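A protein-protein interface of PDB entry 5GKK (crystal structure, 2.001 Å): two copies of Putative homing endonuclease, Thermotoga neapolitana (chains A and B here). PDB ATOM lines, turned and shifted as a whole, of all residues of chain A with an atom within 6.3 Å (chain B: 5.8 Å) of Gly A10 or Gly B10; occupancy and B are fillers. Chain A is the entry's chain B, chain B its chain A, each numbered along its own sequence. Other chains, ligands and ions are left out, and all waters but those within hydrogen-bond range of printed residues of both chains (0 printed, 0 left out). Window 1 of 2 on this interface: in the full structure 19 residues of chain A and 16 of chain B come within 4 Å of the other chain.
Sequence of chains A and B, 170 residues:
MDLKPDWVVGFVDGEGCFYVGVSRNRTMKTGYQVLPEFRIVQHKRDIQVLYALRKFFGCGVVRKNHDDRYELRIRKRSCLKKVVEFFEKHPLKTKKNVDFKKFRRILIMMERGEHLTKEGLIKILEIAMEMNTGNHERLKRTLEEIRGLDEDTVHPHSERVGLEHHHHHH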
ATOM      1  N   PRO A   5      22.681   3.422   6.417  1.00  0.00           N
ATOM      2  CA  PRO A   5      22.715   4.573   7.314  1.00  0.00           C
ATOM      3  C   PRO A   5      22.642   5.908   6.576  1.00  0.00           C
ATOM      4  O   PRO A   5      21.839   6.745   6.973  1.00  0.00           O
ATOM      5  CB  PRO A   5      24.067   4.427   8.011  1.00  0.00           C
ATOM      6  CG  PRO A   5      24.256   2.947   8.077  1.00  0.00           C
ATOM      7  CD  PRO A   5      23.754   2.460   6.736  1.00  0.00           C
ATOM      8  N   ASP A   6      23.446   6.102   5.532  1.00  0.00           N
ATOM      9  CA  ASP A   6      23.436   7.380   4.830  1.00  0.00           C
ATOM     10  C   ASP A   6      22.150   7.586   4.045  1.00  0.00           C
ATOM     11  O   ASP A   6      21.744   8.723   3.790  1.00  0.00           O
ATOM     12  CB  ASP A   6      24.658   7.545   3.942  1.00  0.00           C
ATOM     13  CG  ASP A   6      25.947   7.644   4.745  1.00  0.00           C
ATOM     14  OD1 ASP A   6      25.964   8.406   5.738  1.00  0.00           O
ATOM     15  OD2 ASP A   6      26.933   6.944   4.411  1.00  0.00           O
ATOM     16  N   TRP A   7      21.495   6.491   3.680  1.00  0.00           N
ATOM     17  CA  TRP A   7      20.172   6.609   3.077  1.00  0.00           C
ATOM     18  C   TRP A   7      19.227   7.147   4.147  1.00  0.00           C
ATOM     19  O   TRP A   7      18.457   8.051   3.884  1.00  0.00           O
ATOM     20  CB  TRP A   7      19.663   5.262   2.508  1.00  0.00           C
ATOM     21  CG  TRP A   7      18.326   5.424   1.850  1.00  0.00           C
ATOM     22  CD1 TRP A   7      18.070   5.608   0.504  1.00  0.00           C
ATOM     23  CD2 TRP A   7      17.067   5.481   2.505  1.00  0.00           C
ATOM     24  NE1 TRP A   7      16.720   5.761   0.295  1.00  0.00           N
ATOM     25  CE2 TRP A   7      16.081   5.689   1.506  1.00  0.00           C
ATOM     26  CE3 TRP A   7      16.664   5.359   3.846  1.00  0.00           C
ATOM     27  CZ2 TRP A   7      14.724   5.771   1.809  1.00  0.00           C
ATOM     28  CZ3 TRP A   7      15.316   5.451   4.140  1.00  0.00           C
ATOM     29  CH2 TRP A   7      14.361   5.646   3.124  1.00  0.00           C
ATOM     30  N   VAL A   8      19.298   6.596   5.355  1.00  0.00           N
ATOM     31  CA  VAL A   8      18.456   7.075   6.464  1.00  0.00           C
ATOM     32  C   VAL A   8      18.676   8.576   6.779  1.00  0.00           C
ATOM     33  O   VAL A   8      17.720   9.336   6.949  1.00  0.00           O
ATOM     34  CB  VAL A   8      18.680   6.265   7.764  1.00  0.00           C
ATOM     35  CG1 VAL A   8      17.951   6.955   8.941  1.00  0.00           C
ATOM     36  CG2 VAL A   8      18.227   4.811   7.589  1.00  0.00           C
ATOM     37  N   VAL A   9      19.935   8.986   6.839  1.00  0.00           N
ATOM     38  CA  VAL A   9      20.273  10.413   7.015  1.00  0.00           C
ATOM     39  C   VAL A   9      19.657  11.278   5.905  1.00  0.00           C
ATOM     40  O   VAL A   9      19.027  12.266   6.184  1.00  0.00           O
ATOM     41  CB  VAL A   9      21.794  10.633   7.106  1.00  0.00           C
ATOM     42  CG1 VAL A   9      22.142  12.120   7.320  1.00  0.00           C
ATOM     43  CG2 VAL A   9      22.372   9.784   8.231  1.00  0.00           C
ATOM     44  N   GLY A  10      19.815  10.880   4.647  1.00  0.00           N
ATOM     45  CA  GLY A  10      19.176  11.590   3.552  1.00  0.00           C
ATOM     46  C   GLY A  10      17.660  11.682   3.693  1.00  0.00           C
ATOM     47  O   GLY A  10      17.077  12.759   3.553  1.00  0.00           O
ATOM     48  N   PHE A  11      17.015  10.555   3.986  1.00  0.00           N
ATOM     49  CA  PHE A  11      15.558  10.530   4.079  1.00  0.00           C
ATOM     50  C   PHE A  11      15.042  11.416   5.239  1.00  0.00           C
ATOM     51  O   PHE A  11      13.991  12.081   5.134  1.00  0.00           O
ATOM     52  CB  PHE A  11      15.071   9.100   4.228  1.00  0.00           C
ATOM     53  CG  PHE A  11      13.593   8.950   4.034  1.00  0.00           C
ATOM     54  CD1 PHE A  11      13.037   9.026   2.759  1.00  0.00           C
ATOM     55  CD2 PHE A  11      12.766   8.723   5.110  1.00  0.00           C
ATOM     56  CE1 PHE A  11      11.682   8.882   2.569  1.00  0.00           C
ATOM     57  CE2 PHE A  11      11.403   8.567   4.926  1.00  0.00           C
ATOM     58  CZ  PHE A  11      10.855   8.659   3.659  1.00  0.00           C
ATOM     59  N   VAL A  12      15.797  11.458   6.334  1.00  0.00           N
ATOM     60  CA  VAL A  12      15.378  12.225   7.498  1.00  0.00           C
ATOM     61  C   VAL A  12      15.654  13.726   7.284  1.00  0.00           C
ATOM     62  O   VAL A  12      14.853  14.582   7.690  1.00  0.00           O
ATOM     63  CB  VAL A  12      16.021  11.686   8.807  1.00  0.00           C
ATOM     64  CG1 VAL A  12      15.853  12.702   9.949  1.00  0.00           C
ATOM     65  CG2 VAL A  12      15.383  10.363   9.186  1.00  0.00           C
ATOM     66  N   ASP A  13      16.765  14.048   6.620  1.00  0.00           N
ATOM     67  CA  ASP A  13      17.022  15.427   6.183  1.00  0.00           C
ATOM     68  C   ASP A  13      15.831  15.902   5.351  1.00  0.00           C
ATOM     69  O   ASP A  13      15.430  17.061   5.448  1.00  0.00           O
ATOM     70  CB  ASP A  13      18.299  15.526   5.346  1.00  0.00           C
ATOM     71  CG  ASP A  13      19.518  15.919   6.171  1.00  0.00           C
ATOM     72  OD1 ASP A  13      19.393  16.819   7.047  1.00  0.00           O
ATOM     73  OD2 ASP A  13      20.603  15.333   5.937  1.00  0.00           O
ATOM     74  N   GLY A  14      15.270  14.996   4.544  1.00  0.00           N
ATOM     75  CA  GLY A  14      14.109  15.322   3.731  1.00  0.00           C
ATOM     76  C   GLY A  14      12.777  15.367   4.482  1.00  0.00           C
ATOM     77  O   GLY A  14      12.014  16.355   4.383  1.00  0.00           O
ATOM     78  N   GLU A  15      12.513  14.317   5.259  1.00  0.00           N
ATOM     79  CA  GLU A  15      11.178  14.048   5.803  1.00  0.00           C
ATOM     80  C   GLU A  15      11.043  14.067   7.328  1.00  0.00           C
ATOM     81  O   GLU A  15       9.929  14.018   7.845  1.00  0.00           O
ATOM     82  CB  GLU A  15      10.675  12.693   5.309  1.00  0.00           C
ATOM     83  CG  GLU A  15      10.444  12.588   3.801  1.00  0.00           C
ATOM     84  CD  GLU A  15       9.341  13.515   3.322  1.00  0.00           C
ATOM     85  OE1 GLU A  15       8.212  13.027   3.113  1.00  0.00           O
ATOM     86  OE2 GLU A  15       9.598  14.726   3.155  1.00  0.00           O
ATOM     87  N   LEU A  92      23.170  15.018  10.226  1.00  0.00           N
ATOM     88  CA  LEU A  92      22.268  15.560   9.227  1.00  0.00           C
ATOM     89  C   LEU A  92      22.976  16.622   8.408  1.00  0.00           C
ATOM     90  O   LEU A  92      23.961  17.177   8.840  1.00  0.00           O
ATOM     91  CB  LEU A  92      21.041  16.140   9.907  1.00  0.00           C
ATOM     92  CG  LEU A  92      20.238  15.006  10.538  1.00  0.00           C
ATOM     93  CD1 LEU A  92      19.473  15.453  11.774  1.00  0.00           C
ATOM     94  CD2 LEU A  92      19.302  14.424   9.470  1.00  0.00           C
ATOM     95  N   PRO B   5      26.431   9.464  -2.295  1.00  0.00           N
ATOM     96  CA  PRO B   5      25.375   8.845  -3.120  1.00  0.00           C
ATOM     97  C   PRO B   5      24.187   8.314  -2.319  1.00  0.00           C
ATOM     98  O   PRO B   5      23.052   8.620  -2.648  1.00  0.00           O
ATOM     99  CB  PRO B   5      26.095   7.662  -3.780  1.00  0.00           C
ATOM    100  CG  PRO B   5      27.505   8.074  -3.877  1.00  0.00           C
ATOM    101  CD  PRO B   5      27.778   9.077  -2.754  1.00  0.00           C
ATOM    102  N   ASP B   6      24.432   7.503  -1.298  1.00  0.00           N
ATOM    103  CA  ASP B   6      23.326   6.947  -0.506  1.00  0.00           C
ATOM    104  C   ASP B   6      22.485   8.051   0.156  1.00  0.00           C
ATOM    105  O   ASP B   6      21.268   7.920   0.320  1.00  0.00           O
ATOM    106  CB  ASP B   6      23.864   5.999   0.553  1.00  0.00           C
ATOM    107  CG  ASP B   6      24.355   4.679  -0.040  1.00  0.00           C
ATOM    108  OD1 ASP B   6      23.706   4.161  -0.982  1.00  0.00           O
ATOM    109  OD2 ASP B   6      25.397   4.175   0.431  1.00  0.00           O
ATOM    110  N   TRP B   7      23.146   9.140   0.529  1.00  0.00           N
ATOM    111  CA  TRP B   7      22.440  10.279   1.100  1.00  0.00           C
ATOM    112  C   TRP B   7      21.554  10.927   0.040  1.00  0.00           C
ATOM    113  O   TRP B   7      20.405  11.308   0.305  1.00  0.00           O
ATOM    114  CB  TRP B   7      23.419  11.322   1.663  1.00  0.00           C
ATOM    115  CG  TRP B   7      22.723  12.485   2.353  1.00  0.00           C
ATOM    116  CD1 TRP B   7      22.533  12.641   3.693  1.00  0.00           C
ATOM    117  CD2 TRP B   7      22.142  13.651   1.724  1.00  0.00           C
ATOM    118  NE1 TRP B   7      21.849  13.831   3.943  1.00  0.00           N
ATOM    119  CE2 TRP B   7      21.597  14.454   2.753  1.00  0.00           C
ATOM    120  CE3 TRP B   7      21.988  14.064   0.391  1.00  0.00           C
ATOM    121  CZ2 TRP B   7      20.940  15.656   2.486  1.00  0.00           C
ATOM    122  CZ3 TRP B   7      21.338  15.254   0.129  1.00  0.00           C
ATOM    123  CH2 TRP B   7      20.824  16.041   1.172  1.00  0.00           C
ATOM    124  N   VAL B   8      22.104  11.098  -1.149  1.00  0.00           N
ATOM    125  CA  VAL B   8      21.312  11.631  -2.251  1.00  0.00           C
ATOM    126  C   VAL B   8      20.050  10.787  -2.506  1.00  0.00           C
ATOM    127  O   VAL B   8      18.952  11.324  -2.663  1.00  0.00           O
ATOM    128  CB  VAL B   8      22.134  11.733  -3.526  1.00  0.00           C
ATOM    129  CG1 VAL B   8      21.252  12.145  -4.655  1.00  0.00           C
ATOM    130  CG2 VAL B   8      23.264  12.756  -3.315  1.00  0.00           C
ATOM    131  N   VAL B   9      20.214   9.468  -2.520  1.00  0.00           N
ATOM    132  CA  VAL B   9      19.082   8.572  -2.743  1.00  0.00           C
ATOM    133  C   VAL B   9      18.014   8.813  -1.667  1.00  0.00           C
ATOM    134  O   VAL B   9      16.834   9.013  -1.987  1.00  0.00           O
ATOM    135  CB  VAL B   9      19.526   7.075  -2.771  1.00  0.00           C
ATOM    136  CG1 VAL B   9      18.327   6.139  -2.998  1.00  0.00           C
ATOM    137  CG2 VAL B   9      20.566   6.841  -3.884  1.00  0.00           C
ATOM    138  N   GLY B  10      18.444   8.789  -0.401  1.00  0.00           N
ATOM    139  CA  GLY B  10      17.555   9.007   0.732  1.00  0.00           C
ATOM    140  C   GLY B  10      16.788  10.318   0.603  1.00  0.00           C
ATOM    141  O   GLY B  10      15.562  10.360   0.699  1.00  0.00           O
ATOM    142  N   PHE B  11      17.517  11.390   0.338  1.00  0.00           N
ATOM    143  CA  PHE B  11      16.918  12.707   0.187  1.00  0.00           C
ATOM    144  C   PHE B  11      15.932  12.773  -0.998  1.00  0.00           C
ATOM    145  O   PHE B  11      14.840  13.344  -0.884  1.00  0.00           O
ATOM    146  CB  PHE B  11      18.018  13.764   0.035  1.00  0.00           C
ATOM    147  CG  PHE B  11      17.536  15.186   0.249  1.00  0.00           C
ATOM    148  CD1 PHE B  11      17.244  15.652   1.530  1.00  0.00           C
ATOM    149  CD2 PHE B  11      17.385  16.043  -0.819  1.00  0.00           C
ATOM    150  CE1 PHE B  11      16.812  16.941   1.737  1.00  0.00           C
ATOM    151  CE2 PHE B  11      16.959  17.350  -0.624  1.00  0.00           C
ATOM    152  CZ  PHE B  11      16.670  17.795   0.656  1.00  0.00           C
ATOM    153  N   VAL B  12      16.320  12.207  -2.135  1.00  0.00           N
ATOM    154  CA  VAL B  12      15.453  12.234  -3.301  1.00  0.00           C
ATOM    155  C   VAL B  12      14.242  11.325  -3.068  1.00  0.00           C
ATOM    156  O   VAL B  12      13.128  11.677  -3.445  1.00  0.00           O
ATOM    157  CB  VAL B  12      16.218  11.919  -4.600  1.00  0.00           C
ATOM    158  CG1 VAL B  12      15.265  11.672  -5.776  1.00  0.00           C
ATOM    159  CG2 VAL B  12      17.166  13.047  -4.927  1.00  0.00           C
ATOM    160  N   ASP B  13      14.444  10.188  -2.415  1.00  0.00           N
ATOM    161  CA  ASP B  13      13.308   9.366  -2.012  1.00  0.00           C
ATOM    162  C   ASP B  13      12.288  10.210  -1.255  1.00  0.00           C
ATOM    163  O   ASP B  13      11.082  10.119  -1.504  1.00  0.00           O
ATOM    164  CB  ASP B  13      13.744   8.178  -1.149  1.00  0.00           C
ATOM    165  CG  ASP B  13      13.736   6.862  -1.904  1.00  0.00           C
ATOM    166  OD1 ASP B  13      12.766   6.586  -2.663  1.00  0.00           O
ATOM    167  OD2 ASP B  13      14.709   6.092  -1.729  1.00  0.00           O
ATOM    168  N   GLY B  14      12.772  11.069  -0.368  1.00  0.00           N
ATOM    169  CA  GLY B  14      11.894  11.935   0.393  1.00  0.00           C
ATOM    170  C   GLY B  14      11.358  13.146  -0.373  1.00  0.00           C
ATOM    171  O   GLY B  14      10.155  13.395  -0.386  1.00  0.00           O
ATOM    172  N   GLU B  15      12.238  13.891  -1.035  1.00  0.00           N
ATOM    173  CA  GLU B  15      11.855  15.197  -1.570  1.00  0.00           C
ATOM    174  C   GLU B  15      11.858  15.320  -3.105  1.00  0.00           C
ATOM    175  O   GLU B  15      11.501  16.360  -3.650  1.00  0.00           O
ATOM    176  CB  GLU B  15      12.758  16.281  -0.967  1.00  0.00           C
ATOM    177  CG  GLU B  15      12.559  16.493   0.523  1.00  0.00           C
ATOM    178  CD  GLU B  15      11.253  17.223   0.836  1.00  0.00           C
ATOM    179  OE1 GLU B  15      11.132  18.420   0.487  1.00  0.00           O
ATOM    180  OE2 GLU B  15      10.341  16.602   1.424  1.00  0.00           O
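OE2 of Glu A15 sits close to OE2 of Glu B15 (2.7 Å).
The indole nitrogen of Trp A7 lies within hydrogen-bond range of the side-chain carboxylate of Asp B13, at 2.9 Å.
The backbone carbonyl oxygen (O) of Gly A14 lies close to the side-chain carboxylate (OE2) of Glu B15 (3.4 Å).
OD2 of Asp A13 is in hydrogen-bond range of NE1 of Trp B7 (2.8 Å).
Asp A6 touches Asp B6 (O to O, 3.6 Å).
Asp A6 touches Trp B7 (O to CA, 3.2 Å).
Asp B6 touches Trp A7 (O to CA, 3.2 Å).
Gly A10 touches Trp B7.
Gly A10 touches Gly B10.
O of Gly A10 touches CA of Phe B11, at 3.4 Å.
CA of Phe A11 touches O of Gly B10, 3.4 Å away.
Phe B11 touches Phe A11 (N to N, 3.8 Å).
CD1 of Phe B11 touches N of Gly A14, 3.7 Å away.
CA of Gly B14 touches CG of Glu A15, 3.8 Å away.
Gly A10 touches three residues of chain B.
Of the printed residues of chain A, Gly B14 touches Phe A11 (3.7 Å) and Glu A15 (3.8 Å).
Printed residues of chain A within 4 Å of Asp B13: Trp A7.
The nearest residue of chain A that does not touch Gly B10 is Asp A6 (5.2 Å).
The nearest printed residue of chain A that does not touch Glu B15 is Asp A13 (5.7 Å).
Of the 11 printed residues of chain B, 8 touch a printed residue of chain A.
Printed residues of chain B that touch a printed residue of chain A: Asp B6, Trp B7, Val B9, Gly B10, Phe B11, Asp B13, Gly B14 and Glu B15.
Of the 12 printed residues of chain A, 8 touch a printed residue of chain B.
Hydrophobic or aromatic side chains of chain A within 4 Å of the printed part of chain B: Trp A7, Val A9 and Phe A11.
Along chain A the printed residues that touch a printed residue of chain B span positions 6 to 15.
Among the printed residues, no Asp or Glu carboxylate lies within 4 Å of a Lys or Arg side-chain nitrogen of the other chain.
Asp A6 touches its own counterpart, Asp B6.
Asp A6 touches Trp B7, and with the chains exchanged Trp A7 touches Asp B6.
Trp A7 touches Gly B10, and with the chains exchanged Gly A10 touches Trp B7.
Trp A7 touches Asp B13, and with the chains exchanged Asp A13 touches Trp B7.
Positions printed for both chains: 5, 6, 7, 8, 9, 10, 11, 12, 13, 14 and 15.
Of the 19 pairs that touch across the chains among the printed residues, 18 have their exchanged pair printed and touching as well.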
